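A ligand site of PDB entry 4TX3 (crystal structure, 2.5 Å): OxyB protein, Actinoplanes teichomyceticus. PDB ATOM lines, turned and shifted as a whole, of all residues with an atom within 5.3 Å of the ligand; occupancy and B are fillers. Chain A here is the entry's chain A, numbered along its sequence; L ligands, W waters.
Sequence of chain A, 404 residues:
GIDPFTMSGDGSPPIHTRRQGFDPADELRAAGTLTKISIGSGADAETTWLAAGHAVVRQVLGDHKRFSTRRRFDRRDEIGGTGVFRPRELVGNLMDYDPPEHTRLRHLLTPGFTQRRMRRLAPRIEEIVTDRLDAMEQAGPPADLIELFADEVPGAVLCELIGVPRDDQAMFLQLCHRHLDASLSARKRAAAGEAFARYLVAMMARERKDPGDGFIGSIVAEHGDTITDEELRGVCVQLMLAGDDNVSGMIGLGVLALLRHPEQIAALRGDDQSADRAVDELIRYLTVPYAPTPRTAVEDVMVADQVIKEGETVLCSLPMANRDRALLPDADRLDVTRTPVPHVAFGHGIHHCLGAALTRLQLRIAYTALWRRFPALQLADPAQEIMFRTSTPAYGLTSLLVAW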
ATOM      1  N   LEU A  61     -34.301  12.800 -29.380  1.00  0.00           N
ATOM      2  CA  LEU A  61     -32.916  12.439 -29.077  1.00  0.00           C
ATOM      3  C   LEU A  61     -32.387  11.431 -30.095  1.00  0.00           C
ATOM      4  O   LEU A  61     -31.199  11.448 -30.482  1.00  0.00           O
ATOM      5  CB  LEU A  61     -32.796  11.852 -27.662  1.00  0.00           C
ATOM      6  CG  LEU A  61     -33.274  12.746 -26.504  1.00  0.00           C
ATOM      7  CD1 LEU A  61     -33.235  11.966 -25.189  1.00  0.00           C
ATOM      8  CD2 LEU A  61     -32.455  14.041 -26.403  1.00  0.00           C
ATOM      9  N   LEU A  94     -18.394  16.516 -26.635  1.00  0.00           N
ATOM     10  CA  LEU A  94     -19.171  15.711 -27.588  1.00  0.00           C
ATOM     11  C   LEU A  94     -20.616  16.117 -27.704  1.00  0.00           C
ATOM     12  O   LEU A  94     -21.218  15.969 -28.769  1.00  0.00           O
ATOM     13  CB  LEU A  94     -19.125  14.228 -27.191  1.00  0.00           C
ATOM     14  CG  LEU A  94     -17.967  13.406 -27.771  1.00  0.00           C
ATOM     15  CD1 LEU A  94     -16.662  14.106 -27.529  1.00  0.00           C
ATOM     16  CD2 LEU A  94     -17.915  12.020 -27.140  1.00  0.00           C
ATOM     17  N   MET A  95     -21.191  16.639 -26.627  1.00  0.00           N
ATOM     18  CA  MET A  95     -22.568  17.123 -26.653  1.00  0.00           C
ATOM     19  C   MET A  95     -22.778  18.260 -27.665  1.00  0.00           C
ATOM     20  O   MET A  95     -23.893  18.509 -28.085  1.00  0.00           O
ATOM     21  CB  MET A  95     -23.010  17.591 -25.264  1.00  0.00           C
ATOM     22  CG  MET A  95     -23.331  16.466 -24.286  1.00  0.00           C
ATOM     23  SD  MET A  95     -23.735  17.081 -22.636  1.00  0.00           S
ATOM     24  CE  MET A  95     -22.451  16.316 -21.627  1.00  0.00           C
ATOM     25  N   HIS A 102     -18.888  14.349 -34.516  1.00  0.00           N
ATOM     26  CA  HIS A 102     -19.215  13.633 -33.286  1.00  0.00           C
ATOM     27  C   HIS A 102     -18.831  12.158 -33.356  1.00  0.00           C
ATOM     28  O   HIS A 102     -18.359  11.587 -32.367  1.00  0.00           O
ATOM     29  CB  HIS A 102     -20.702  13.723 -32.978  1.00  0.00           C
ATOM     30  CG  HIS A 102     -21.146  12.823 -31.877  1.00  0.00           C
ATOM     31  ND1 HIS A 102     -21.499  11.497 -32.071  1.00  0.00           N
ATOM     32  CD2 HIS A 102     -21.275  13.041 -30.544  1.00  0.00           C
ATOM     33  CE1 HIS A 102     -21.824  10.959 -30.917  1.00  0.00           C
ATOM     34  NE2 HIS A 102     -21.707  11.874 -29.972  1.00  0.00           N
ATOM     35  N   ARG A 106     -15.973  10.702 -30.747  1.00  0.00           N
ATOM     36  CA  ARG A 106     -16.471   9.721 -29.793  1.00  0.00           C
ATOM     37  C   ARG A 106     -15.756   8.393 -30.003  1.00  0.00           C
ATOM     38  O   ARG A 106     -15.381   7.718 -29.039  1.00  0.00           O
ATOM     39  CB  ARG A 106     -17.995   9.570 -29.910  1.00  0.00           C
ATOM     40  CG  ARG A 106     -18.567   8.416 -29.117  1.00  0.00           C
ATOM     41  CD  ARG A 106     -19.809   8.815 -28.351  1.00  0.00           C
ATOM     42  NE  ARG A 106     -20.258   7.710 -27.510  1.00  0.00           N
ATOM     43  CZ  ARG A 106     -21.291   7.759 -26.674  1.00  0.00           C
ATOM     44  NH1 ARG A 106     -21.997   8.872 -26.554  1.00  0.00           N
ATOM     45  NH2 ARG A 106     -21.597   6.688 -25.955  1.00  0.00           N
ATOM     46  N   PHE A 113     -12.583   3.388 -22.380  1.00  0.00           N
ATOM     47  CA  PHE A 113     -13.891   3.078 -21.816  1.00  0.00           C
ATOM     48  C   PHE A 113     -14.301   1.601 -21.948  1.00  0.00           C
ATOM     49  O   PHE A 113     -15.465   1.247 -21.670  1.00  0.00           O
ATOM     50  CB  PHE A 113     -14.948   3.952 -22.488  1.00  0.00           C
ATOM     51  CG  PHE A 113     -15.093   5.316 -21.886  1.00  0.00           C
ATOM     52  CD1 PHE A 113     -15.805   5.497 -20.708  1.00  0.00           C
ATOM     53  CD2 PHE A 113     -14.522   6.426 -22.510  1.00  0.00           C
ATOM     54  CE1 PHE A 113     -15.949   6.754 -20.157  1.00  0.00           C
ATOM     55  CE2 PHE A 113     -14.659   7.689 -21.962  1.00  0.00           C
ATOM     56  CZ  PHE A 113     -15.365   7.858 -20.789  1.00  0.00           C
ATOM     57  N   LEU A 158     -13.459  10.009 -11.287  1.00  0.00           N
ATOM     58  CA  LEU A 158     -13.049  10.696 -12.501  1.00  0.00           C
ATOM     59  C   LEU A 158     -11.524  10.899 -12.594  1.00  0.00           C
ATOM     60  O   LEU A 158     -10.945  10.719 -13.660  1.00  0.00           O
ATOM     61  CB  LEU A 158     -13.758  12.046 -12.589  1.00  0.00           C
ATOM     62  CG  LEU A 158     -15.233  11.925 -12.987  1.00  0.00           C
ATOM     63  CD1 LEU A 158     -15.921  13.254 -12.908  1.00  0.00           C
ATOM     64  CD2 LEU A 158     -15.320  11.357 -14.387  1.00  0.00           C
ATOM     65  N   LEU A 161     -10.179   7.607 -13.698  1.00  0.00           N
ATOM     66  CA  LEU A 161     -10.527   7.341 -15.077  1.00  0.00           C
ATOM     67  C   LEU A 161      -9.487   7.979 -15.990  1.00  0.00           C
ATOM     68  O   LEU A 161      -8.926   7.289 -16.819  1.00  0.00           O
ATOM     69  CB  LEU A 161     -11.938   7.877 -15.382  1.00  0.00           C
ATOM     70  CG  LEU A 161     -12.388   7.847 -16.846  1.00  0.00           C
ATOM     71  CD1 LEU A 161     -12.508   6.421 -17.341  1.00  0.00           C
ATOM     72  CD2 LEU A 161     -13.704   8.578 -16.994  1.00  0.00           C
ATOM     73  N   LEU A 239     -14.957  15.826 -19.390  1.00  0.00           N
ATOM     74  CA  LEU A 239     -15.220  14.628 -18.616  1.00  0.00           C
ATOM     75  C   LEU A 239     -15.417  15.017 -17.163  1.00  0.00           C
ATOM     76  O   LEU A 239     -16.345  14.525 -16.500  1.00  0.00           O
ATOM     77  CB  LEU A 239     -14.091  13.611 -18.778  1.00  0.00           C
ATOM     78  CG  LEU A 239     -14.095  12.873 -20.110  1.00  0.00           C
ATOM     79  CD1 LEU A 239     -12.995  11.841 -20.167  1.00  0.00           C
ATOM     80  CD2 LEU A 239     -15.461  12.228 -20.337  1.00  0.00           C
ATOM     81  N   ALA A 242     -18.743  16.651 -16.760  1.00  0.00           N
ATOM     82  CA  ALA A 242     -19.913  15.846 -17.131  1.00  0.00           C
ATOM     83  C   ALA A 242     -20.265  14.788 -16.088  1.00  0.00           C
ATOM     84  O   ALA A 242     -21.437  14.436 -15.928  1.00  0.00           O
ATOM     85  CB  ALA A 242     -19.700  15.185 -18.485  1.00  0.00           C
ATOM     86  N   GLY A 243     -19.268  14.281 -15.383  1.00  0.00           N
ATOM     87  CA  GLY A 243     -19.484  13.139 -14.517  1.00  0.00           C
ATOM     88  C   GLY A 243     -19.408  13.343 -13.018  1.00  0.00           C
ATOM     89  O   GLY A 243     -19.283  12.375 -12.262  1.00  0.00           O
ATOM     90  N   ASN A 246     -23.708  15.059 -11.695  1.00  0.00           N
ATOM     91  CA  ASN A 246     -24.718  14.034 -11.899  1.00  0.00           C
ATOM     92  C   ASN A 246     -24.623  12.885 -10.887  1.00  0.00           C
ATOM     93  O   ASN A 246     -25.639  12.462 -10.322  1.00  0.00           O
ATOM     94  CB  ASN A 246     -24.629  13.451 -13.297  1.00  0.00           C
ATOM     95  CG  ASN A 246     -25.285  14.323 -14.326  1.00  0.00           C
ATOM     96  OD1 ASN A 246     -24.820  14.407 -15.460  1.00  0.00           O
ATOM     97  ND2 ASN A 246     -26.352  14.995 -13.951  1.00  0.00           N
ATOM     98  N   VAL A 247     -23.415  12.388 -10.681  1.00  0.00           N
ATOM     99  CA  VAL A 247     -23.240  11.287  -9.760  1.00  0.00           C
ATOM    100  C   VAL A 247     -23.468  11.759  -8.323  1.00  0.00           C
ATOM    101  O   VAL A 247     -24.102  11.043  -7.530  1.00  0.00           O
ATOM    102  CB  VAL A 247     -21.843  10.660  -9.906  1.00  0.00           C
ATOM    103  CG1 VAL A 247     -21.677   9.504  -8.927  1.00  0.00           C
ATOM    104  CG2 VAL A 247     -21.665  10.166 -11.315  1.00  0.00           C
ATOM    105  N   MET A 250     -27.034  11.851  -7.558  1.00  0.00           N
ATOM    106  CA  MET A 250     -27.578  10.496  -7.454  1.00  0.00           C
ATOM    107  C   MET A 250     -27.255   9.884  -6.103  1.00  0.00           C
ATOM    108  O   MET A 250     -28.131   9.293  -5.462  1.00  0.00           O
ATOM    109  CB  MET A 250     -27.051   9.610  -8.584  1.00  0.00           C
ATOM    110  CG  MET A 250     -27.824   9.732  -9.871  1.00  0.00           C
ATOM    111  SD  MET A 250     -29.557   9.209  -9.677  1.00  0.00           S
ATOM    112  CE  MET A 250     -29.375   7.571  -9.011  1.00  0.00           C
ATOM    113  N   VAL A 288     -31.887  12.788 -12.233  1.00  0.00           N
ATOM    114  CA  VAL A 288     -31.379  14.042 -11.716  1.00  0.00           C
ATOM    115  C   VAL A 288     -31.111  15.117 -12.791  1.00  0.00           C
ATOM    116  O   VAL A 288     -31.289  16.285 -12.489  1.00  0.00           O
ATOM    117  CB  VAL A 288     -30.110  13.828 -10.817  1.00  0.00           C
ATOM    118  CG1 VAL A 288     -30.354  12.686  -9.819  1.00  0.00           C
ATOM    119  CG2 VAL A 288     -28.803  13.600 -11.598  1.00  0.00           C
ATOM    120  N   PRO A 289     -30.727  14.748 -14.039  1.00  0.00           N
ATOM    121  CA  PRO A 289     -30.633  15.866 -14.992  1.00  0.00           C
ATOM    122  C   PRO A 289     -32.005  16.371 -15.504  1.00  0.00           C
ATOM    123  O   PRO A 289     -32.863  15.569 -15.900  1.00  0.00           O
ATOM    124  CB  PRO A 289     -29.798  15.300 -16.134  1.00  0.00           C
ATOM    125  CG  PRO A 289     -29.986  13.847 -16.066  1.00  0.00           C
ATOM    126  CD  PRO A 289     -30.215  13.492 -14.641  1.00  0.00           C
ATOM    127  N   PRO A 292     -31.460  17.351 -21.466  1.00  0.00           N
ATOM    128  CA  PRO A 292     -30.249  17.169 -22.261  1.00  0.00           C
ATOM    129  C   PRO A 292     -29.917  18.476 -22.976  1.00  0.00           C
ATOM    130  O   PRO A 292     -30.564  19.493 -22.751  1.00  0.00           O
ATOM    131  CB  PRO A 292     -30.644  16.085 -23.256  1.00  0.00           C
ATOM    132  CG  PRO A 292     -32.101  16.276 -23.449  1.00  0.00           C
ATOM    133  CD  PRO A 292     -32.642  16.759 -22.124  1.00  0.00           C
ATOM    134  N   THR A 293     -28.912  18.430 -23.837  1.00  0.00           N
ATOM    135  CA  THR A 293     -28.559  19.600 -24.608  1.00  0.00           C
ATOM    136  C   THR A 293     -29.776  19.993 -25.457  1.00  0.00           C
ATOM    137  O   THR A 293     -30.462  19.120 -25.993  1.00  0.00           O
ATOM    138  CB  THR A 293     -27.339  19.331 -25.514  1.00  0.00           C
ATOM    139  OG1 THR A 293     -26.329  18.646 -24.758  1.00  0.00           O
ATOM    140  CG2 THR A 293     -26.773  20.633 -26.046  1.00  0.00           C
ATOM    141  N   ARG A 295     -32.077  20.916 -28.510  1.00  0.00           N
ATOM    142  CA  ARG A 295     -31.987  20.484 -29.896  1.00  0.00           C
ATOM    143  C   ARG A 295     -32.502  21.585 -30.815  1.00  0.00           C
ATOM    144  O   ARG A 295     -33.388  22.353 -30.447  1.00  0.00           O
ATOM    145  CB  ARG A 295     -32.778  19.200 -30.135  1.00  0.00           C
ATOM    146  CG  ARG A 295     -31.923  17.941 -30.158  1.00  0.00           C
ATOM    147  CD  ARG A 295     -31.256  17.671 -28.821  1.00  0.00           C
ATOM    148  NE  ARG A 295     -30.507  16.412 -28.840  1.00  0.00           N
ATOM    149  CZ  ARG A 295     -29.824  15.937 -27.801  1.00  0.00           C
ATOM    150  NH1 ARG A 295     -29.803  16.609 -26.664  1.00  0.00           N
ATOM    151  NH2 ARG A 295     -29.169  14.780 -27.903  1.00  0.00           N
ATOM    152  N   LEU A 318     -36.411  15.264 -19.233  1.00  0.00           N
ATOM    153  CA  LEU A 318     -36.084  13.886 -18.901  1.00  0.00           C
ATOM    154  C   LEU A 318     -36.898  13.335 -17.685  1.00  0.00           C
ATOM    155  O   LEU A 318     -37.355  12.193 -17.754  1.00  0.00           O
ATOM    156  CB  LEU A 318     -34.575  13.735 -18.652  1.00  0.00           C
ATOM    157  CG  LEU A 318     -33.655  14.150 -19.810  1.00  0.00           C
ATOM    158  CD1 LEU A 318     -32.193  14.018 -19.418  1.00  0.00           C
ATOM    159  CD2 LEU A 318     -33.938  13.342 -21.076  1.00  0.00           C
ATOM    160  N   VAL A 344     -34.832   7.446 -20.071  1.00  0.00           N
ATOM    161  CA  VAL A 344     -33.913   8.321 -20.762  1.00  0.00           C
ATOM    162  C   VAL A 344     -33.089   9.218 -19.845  1.00  0.00           C
ATOM    163  O   VAL A 344     -32.661  10.296 -20.266  1.00  0.00           O
ATOM    164  CB  VAL A 344     -34.659   9.220 -21.769  1.00  0.00           C
ATOM    165  CG1 VAL A 344     -35.298   8.362 -22.848  1.00  0.00           C
ATOM    166  CG2 VAL A 344     -35.714  10.080 -21.040  1.00  0.00           C
ATOM    167  N   ALA A 345     -32.850   8.774 -18.619  1.00  0.00           N
ATOM    168  CA  ALA A 345     -32.024   9.567 -17.695  1.00  0.00           C
ATOM    169  C   ALA A 345     -30.579   9.646 -18.203  1.00  0.00           C
ATOM    170  O   ALA A 345     -29.855  10.586 -17.864  1.00  0.00           O
ATOM    171  CB  ALA A 345     -32.066   8.994 -16.283  1.00  0.00           C
ATOM    172  N   PHE A 346     -30.159   8.678 -19.005  1.00  0.00           N
ATOM    173  CA  PHE A 346     -28.817   8.686 -19.582  1.00  0.00           C
ATOM    174  C   PHE A 346     -28.877   9.201 -21.013  1.00  0.00           C
ATOM    175  O   PHE A 346     -27.904   9.087 -21.771  1.00  0.00           O
ATOM    176  CB  PHE A 346     -28.188   7.291 -19.558  1.00  0.00           C
ATOM    177  CG  PHE A 346     -27.548   6.925 -18.231  1.00  0.00           C
ATOM    178  CD1 PHE A 346     -26.677   7.800 -17.597  1.00  0.00           C
ATOM    179  CD2 PHE A 346     -27.820   5.691 -17.635  1.00  0.00           C
ATOM    180  CE1 PHE A 346     -26.078   7.460 -16.391  1.00  0.00           C
ATOM    181  CE2 PHE A 346     -27.243   5.340 -16.434  1.00  0.00           C
ATOM    182  CZ  PHE A 346     -26.350   6.238 -15.803  1.00  0.00           C
ATOM    183  N   GLY A 347     -30.005   9.761 -21.392  1.00  0.00           N
ATOM    184  CA  GLY A 347     -30.206  10.154 -22.776  1.00  0.00           C
ATOM    185  C   GLY A 347     -30.535   8.957 -23.654  1.00  0.00           C
ATOM    186  O   GLY A 347     -30.934   7.896 -23.150  1.00  0.00           O
ATOM    187  N   ILE A 350     -27.141   8.830 -30.214  1.00  0.00           N
ATOM    188  CA  ILE A 350     -25.714   8.935 -30.430  1.00  0.00           C
ATOM    189  C   ILE A 350     -25.011   9.647 -29.285  1.00  0.00           C
ATOM    190  O   ILE A 350     -23.817   9.452 -29.079  1.00  0.00           O
ATOM    191  CB  ILE A 350     -25.409   9.648 -31.786  1.00  0.00           C
ATOM    192  CG1 ILE A 350     -25.858  11.106 -31.762  1.00  0.00           C
ATOM    193  CG2 ILE A 350     -26.073   8.877 -32.942  1.00  0.00           C
ATOM    194  CD1 ILE A 350     -25.341  11.918 -32.930  1.00  0.00           C
ATOM    195  N   HIS A 351     -25.758  10.454 -28.511  1.00  0.00           N
ATOM    196  CA  HIS A 351     -25.152  11.220 -27.420  1.00  0.00           C
ATOM    197  C   HIS A 351     -25.336  10.520 -26.076  1.00  0.00           C
ATOM    198  O   HIS A 351     -24.954  11.068 -25.029  1.00  0.00           O
ATOM    199  CB  HIS A 351     -25.722  12.636 -27.353  1.00  0.00           C
ATOM    200  CG  HIS A 351     -25.324  13.500 -28.514  1.00  0.00           C
ATOM    201  ND1 HIS A 351     -24.045  14.004 -28.666  1.00  0.00           N
ATOM    202  CD2 HIS A 351     -26.017  13.915 -29.609  1.00  0.00           C
ATOM    203  CE1 HIS A 351     -23.974  14.698 -29.790  1.00  0.00           C
ATOM    204  NE2 HIS A 351     -25.155  14.658 -30.368  1.00  0.00           N
ATOM    205  N   HIS A 352     -25.929   9.320 -26.127  1.00  0.00           N
ATOM    206  CA  HIS A 352     -26.163   8.498 -24.953  1.00  0.00           C
ATOM    207  C   HIS A 352     -24.947   8.483 -24.022  1.00  0.00           C
ATOM    208  O   HIS A 352     -23.805   8.308 -24.465  1.00  0.00           O
ATOM    209  CB  HIS A 352     -26.516   7.068 -25.353  1.00  0.00           C
ATOM    210  CG  HIS A 352     -26.725   6.158 -24.184  1.00  0.00           C
ATOM    211  ND1 HIS A 352     -25.703   5.453 -23.592  1.00  0.00           N
ATOM    212  CD2 HIS A 352     -27.842   5.848 -23.485  1.00  0.00           C
ATOM    213  CE1 HIS A 352     -26.180   4.746 -22.587  1.00  0.00           C
ATOM    214  NE2 HIS A 352     -27.485   4.960 -22.505  1.00  0.00           N
ATOM    215  N   CYS A 353     -25.220   8.664 -22.731  1.00  0.00           N
ATOM    216  CA  CYS A 353     -24.192   8.974 -21.761  1.00  0.00           C
ATOM    217  C   CYS A 353     -22.943   8.092 -21.859  1.00  0.00           C
ATOM    218  O   CYS A 353     -22.998   6.870 -21.692  1.00  0.00           O
ATOM    219  CB  CYS A 353     -24.768   8.892 -20.341  1.00  0.00           C
ATOM    220  SG  CYS A 353     -23.478   9.048 -19.118  1.00  0.00           S
ATOM    221  N   LEU A 354     -21.813   8.742 -22.109  1.00  0.00           N
ATOM    222  CA  LEU A 354     -20.555   8.031 -22.279  1.00  0.00           C
ATOM    223  C   LEU A 354     -20.068   7.430 -20.964  1.00  0.00           C
ATOM    224  O   LEU A 354     -19.297   6.464 -20.979  1.00  0.00           O
ATOM    225  CB  LEU A 354     -19.512   8.970 -22.873  1.00  0.00           C
ATOM    226  CG  LEU A 354     -18.126   8.416 -23.170  1.00  0.00           C
ATOM    227  CD1 LEU A 354     -18.208   7.241 -24.166  1.00  0.00           C
ATOM    228  CD2 LEU A 354     -17.187   9.518 -23.673  1.00  0.00           C
ATOM    229  N   GLY A 355     -20.507   7.988 -19.832  1.00  0.00           N
ATOM    230  CA  GLY A 355     -20.159   7.435 -18.531  1.00  0.00           C
ATOM    231  C   GLY A 355     -21.233   6.581 -17.871  1.00  0.00           C
ATOM    232  O   GLY A 355     -21.260   6.452 -16.643  1.00  0.00           O
ATOM    233  N   LEU A 358     -19.733   3.352 -16.139  1.00  0.00           N
ATOM    234  CA  LEU A 358     -18.965   3.829 -15.003  1.00  0.00           C
ATOM    235  C   LEU A 358     -19.880   4.349 -13.901  1.00  0.00           C
ATOM    236  O   LEU A 358     -19.614   4.131 -12.711  1.00  0.00           O
ATOM    237  CB  LEU A 358     -17.983   4.924 -15.433  1.00  0.00           C
ATOM    238  CG  LEU A 358     -17.101   5.542 -14.344  1.00  0.00           C
ATOM    239  CD1 LEU A 358     -16.246   4.489 -13.693  1.00  0.00           C
ATOM    240  CD2 LEU A 358     -16.248   6.647 -14.928  1.00  0.00           C
ATOM    241  N   THR A 359     -20.951   5.033 -14.276  1.00  0.00           N
ATOM    242  CA  THR A 359     -21.934   5.476 -13.288  1.00  0.00           C
ATOM    243  C   THR A 359     -22.586   4.295 -12.557  1.00  0.00           C
ATOM    244  O   THR A 359     -22.684   4.302 -11.318  1.00  0.00           O
ATOM    245  CB  THR A 359     -23.034   6.327 -13.921  1.00  0.00           C
ATOM    246  OG1 THR A 359     -22.452   7.513 -14.463  1.00  0.00           O
ATOM    247  CG2 THR A 359     -24.049   6.712 -12.894  1.00  0.00           C
ATOM    248  N   GLN A 362     -19.942   2.687 -10.115  1.00  0.00           N
ATOM    249  CA  GLN A 362     -19.798   3.554  -8.952  1.00  0.00           C
ATOM    250  C   GLN A 362     -20.945   3.435  -8.006  1.00  0.00           C
ATOM    251  O   GLN A 362     -20.752   3.336  -6.806  1.00  0.00           O
ATOM    252  CB  GLN A 362     -19.781   5.022  -9.354  1.00  0.00           C
ATOM    253  CG  GLN A 362     -18.529   5.596  -9.822  1.00  0.00           C
ATOM    254  CD  GLN A 362     -18.709   7.075 -10.010  1.00  0.00           C
ATOM    255  OE1 GLN A 362     -18.755   7.835  -9.032  1.00  0.00           O
ATOM    256  NE2 GLN A 362     -18.943   7.485 -11.250  1.00  0.00           N
ATOM    257  N   LEU A 363     -22.137   3.590  -8.554  1.00  0.00           N
ATOM    258  CA  LEU A 363     -23.337   3.701  -7.738  1.00  0.00           C
ATOM    259  C   LEU A 363     -23.599   2.384  -7.008  1.00  0.00           C
ATOM    260  O   LEU A 363     -24.059   2.387  -5.870  1.00  0.00           O
ATOM    261  CB  LEU A 363     -24.539   4.123  -8.594  1.00  0.00           C
ATOM    262  CG  LEU A 363     -24.486   5.599  -9.049  1.00  0.00           C
ATOM    263  CD1 LEU A 363     -25.740   5.960  -9.806  1.00  0.00           C
ATOM    264  CD2 LEU A 363     -24.325   6.521  -7.850  1.00  0.00           C
HETATM  265  C1  LIG L   1     -24.068  12.485 -22.019  1.00  0.00           C
HETATM  266  C2  LIG L   1     -26.722  12.169 -17.939  1.00  0.00           C
HETATM  267  C3  LIG L   1     -22.779  10.622 -15.527  1.00  0.00           C
HETATM  268  C4  LIG L   1     -20.036  11.817 -19.371  1.00  0.00           C
HETATM  269  C5  LIG L   1     -25.132  12.481 -21.137  1.00  0.00           C
HETATM  270  C6  LIG L   1     -26.531  12.723 -21.483  1.00  0.00           C
HETATM  271  C7  LIG L   1     -27.251  12.635 -20.348  1.00  0.00           C
HETATM  272  C8  LIG L   1     -26.353  12.343 -19.255  1.00  0.00           C
HETATM  273  C9  LIG L   1     -28.770  12.815 -20.178  1.00  0.00           C
HETATM  274  C10 LIG L   1     -27.034  13.018 -22.912  1.00  0.00           C
HETATM  275  C11 LIG L   1     -27.079  14.514 -23.129  1.00  0.00           C
HETATM  276  C12 LIG L   1     -27.727  14.870 -24.460  1.00  0.00           C
HETATM  277  O1  LIG L   1     -27.920  16.091 -24.687  1.00  0.00           O
HETATM  278  O2  LIG L   1     -28.055  13.964 -25.273  1.00  0.00           O
HETATM  279  C13 LIG L   1     -25.923  11.611 -16.958  1.00  0.00           C
HETATM  280  C14 LIG L   1     -26.386  11.013 -15.738  1.00  0.00           C
HETATM  281  C15 LIG L   1     -25.319  10.601 -15.049  1.00  0.00           C
HETATM  282  C16 LIG L   1     -24.113  10.882 -15.827  1.00  0.00           C
HETATM  283  C17 LIG L   1     -27.841  10.876 -15.230  1.00  0.00           C
HETATM  284  C18 LIG L   1     -25.551   9.920 -13.691  1.00  0.00           C
HETATM  285  C19 LIG L   1     -24.659   9.947 -12.715  1.00  0.00           C
HETATM  286  C20 LIG L   1     -21.686  10.784 -16.356  1.00  0.00           C
HETATM  287  C21 LIG L   1     -20.297  10.363 -16.134  1.00  0.00           C
HETATM  288  C22 LIG L   1     -19.577  10.715 -17.221  1.00  0.00           C
HETATM  289  C23 LIG L   1     -20.464  11.350 -18.152  1.00  0.00           C
HETATM  290  C24 LIG L   1     -19.781   9.654 -14.870  1.00  0.00           C
HETATM  291  C25 LIG L   1     -18.079  10.577 -17.606  1.00  0.00           C
HETATM  292  C26 LIG L   1     -17.134  10.006 -16.859  1.00  0.00           C
HETATM  293  C27 LIG L   1     -20.820  12.126 -20.455  1.00  0.00           C
HETATM  294  C28 LIG L   1     -20.346  12.553 -21.746  1.00  0.00           C
HETATM  295  C29 LIG L   1     -21.622  12.764 -22.585  1.00  0.00           C
HETATM  296  C30 LIG L   1     -22.730  12.444 -21.703  1.00  0.00           C
HETATM  297  C31 LIG L   1     -18.887  12.750 -22.186  1.00  0.00           C
HETATM  298  C32 LIG L   1     -21.706  13.219 -24.048  1.00  0.00           C
HETATM  299  C33 LIG L   1     -21.769  11.987 -24.961  1.00  0.00           C
HETATM  300  C34 LIG L   1     -21.926  12.404 -26.410  1.00  0.00           C
HETATM  301  O3  LIG L   1     -21.541  11.610 -27.309  1.00  0.00           O
HETATM  302  O4  LIG L   1     -22.429  13.523 -26.703  1.00  0.00           O
HETATM  303  N1  LIG L   1     -25.065  12.252 -19.768  1.00  0.00           N
HETATM  304  N2  LIG L   1     -24.541  11.511 -16.985  1.00  0.00           N
HETATM  305  N3  LIG L   1     -21.726  11.375 -17.611  1.00  0.00           N
HETATM  306  N4  LIG L   1     -22.211  12.066 -20.470  1.00  0.00           N
HETATM  307 FE1  LIG L   1     -23.408  11.580 -18.796  1.00  0.00          FE
HETATM  308  O   HOH W   1     -28.908  11.348 -25.630  1.00  0.00           O
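The side-chain sulfur of Cys 353 lies close to the backbone NH of Gly 355 (3.2 Å).
A ring nitrogen (NE2) of His 102 lies within hydrogen-bond range of a ring nitrogen (ND1) of His 351 (3.4 Å).
The backbone carbonyl oxygen (O) of Thr 293 sits at hydrogen-bond distance from the guanidinium group (NH1) of Arg 295 (2.7 Å).
SD of Met 95 lies close to OG1 of Thr 293 (3.7 Å).
A ring nitrogen (NE2) of His 102 lies close to the backbone carbonyl oxygen (O) of Ile 350, 3.3 Å away.
NH1 of Arg 106 lies within hydrogen-bond range of O of Ile 350, 3.2 Å away.
NH1 of Arg 106 is in hydrogen-bond range of O of His 352 (2.8 Å).
The side-chain hydroxyl (OG1) of Thr 359 sits at hydrogen-bond distance from the backbone carbonyl oxygen (O) of Gly 355, at 2.7 Å.
An iron atom (FE1) of the ligand is bound by the side-chain sulfur (SG) of Cys 353 (2.6 Å).
An oxygen (O4) of the ligand sits at hydrogen-bond distance from a ring nitrogen (ND1) of His 351, at 2.6 Å.
N of Thr 293 lies within hydrogen-bond range of O1 of the ligand (2.7 Å).
O1 of the ligand is in hydrogen-bond range of OG1 of Thr 293 (3.0 Å).
O3 of the ligand is in hydrogen-bond range of NE2 of His 102, 2.7 Å away.
The guanidinium group of Arg 295 is in salt-bridge range of an oxygen (O1) of the ligand, at 2.8 Å.
An oxygen (O3) of the ligand lies within salt-bridge range of the guanidinium group (NH1) of Arg 106, at 2.9 Å.
An oxygen (O4) of the ligand is in hydrogen-bond range of the backbone NH (N) of Met 95, 3.4 Å away.
The backbone carbonyl oxygen of Leu 94 sits close to an oxygen (O4) of the ligand.
OD1 of Asn 246 lies close to N2 of the ligand, 3.3 Å away.
Residues that only touch the ligand: Leu 158, Leu 161, Leu 239, Ala 242, Gly 243, Val 247, Pro 289, Pro 292, Leu 318, Ala 345, Phe 346, Gly 347, Ile 350, Leu 354, Gly 355, Leu 358 and Thr 359.
26 residues have an atom within 4 Å of the ligand: Leu 94, Met 95, His 102, Arg 106, Leu 158, Leu 161, Leu 239, Ala 242, Gly 243, Asn 246, Val 247, Pro 289, Pro 292, Thr 293, Arg 295, Leu 318, Ala 345, Phe 346, Gly 347, Ile 350, His 351, Cys 353, Leu 354, Gly 355, Leu 358 and Thr 359.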
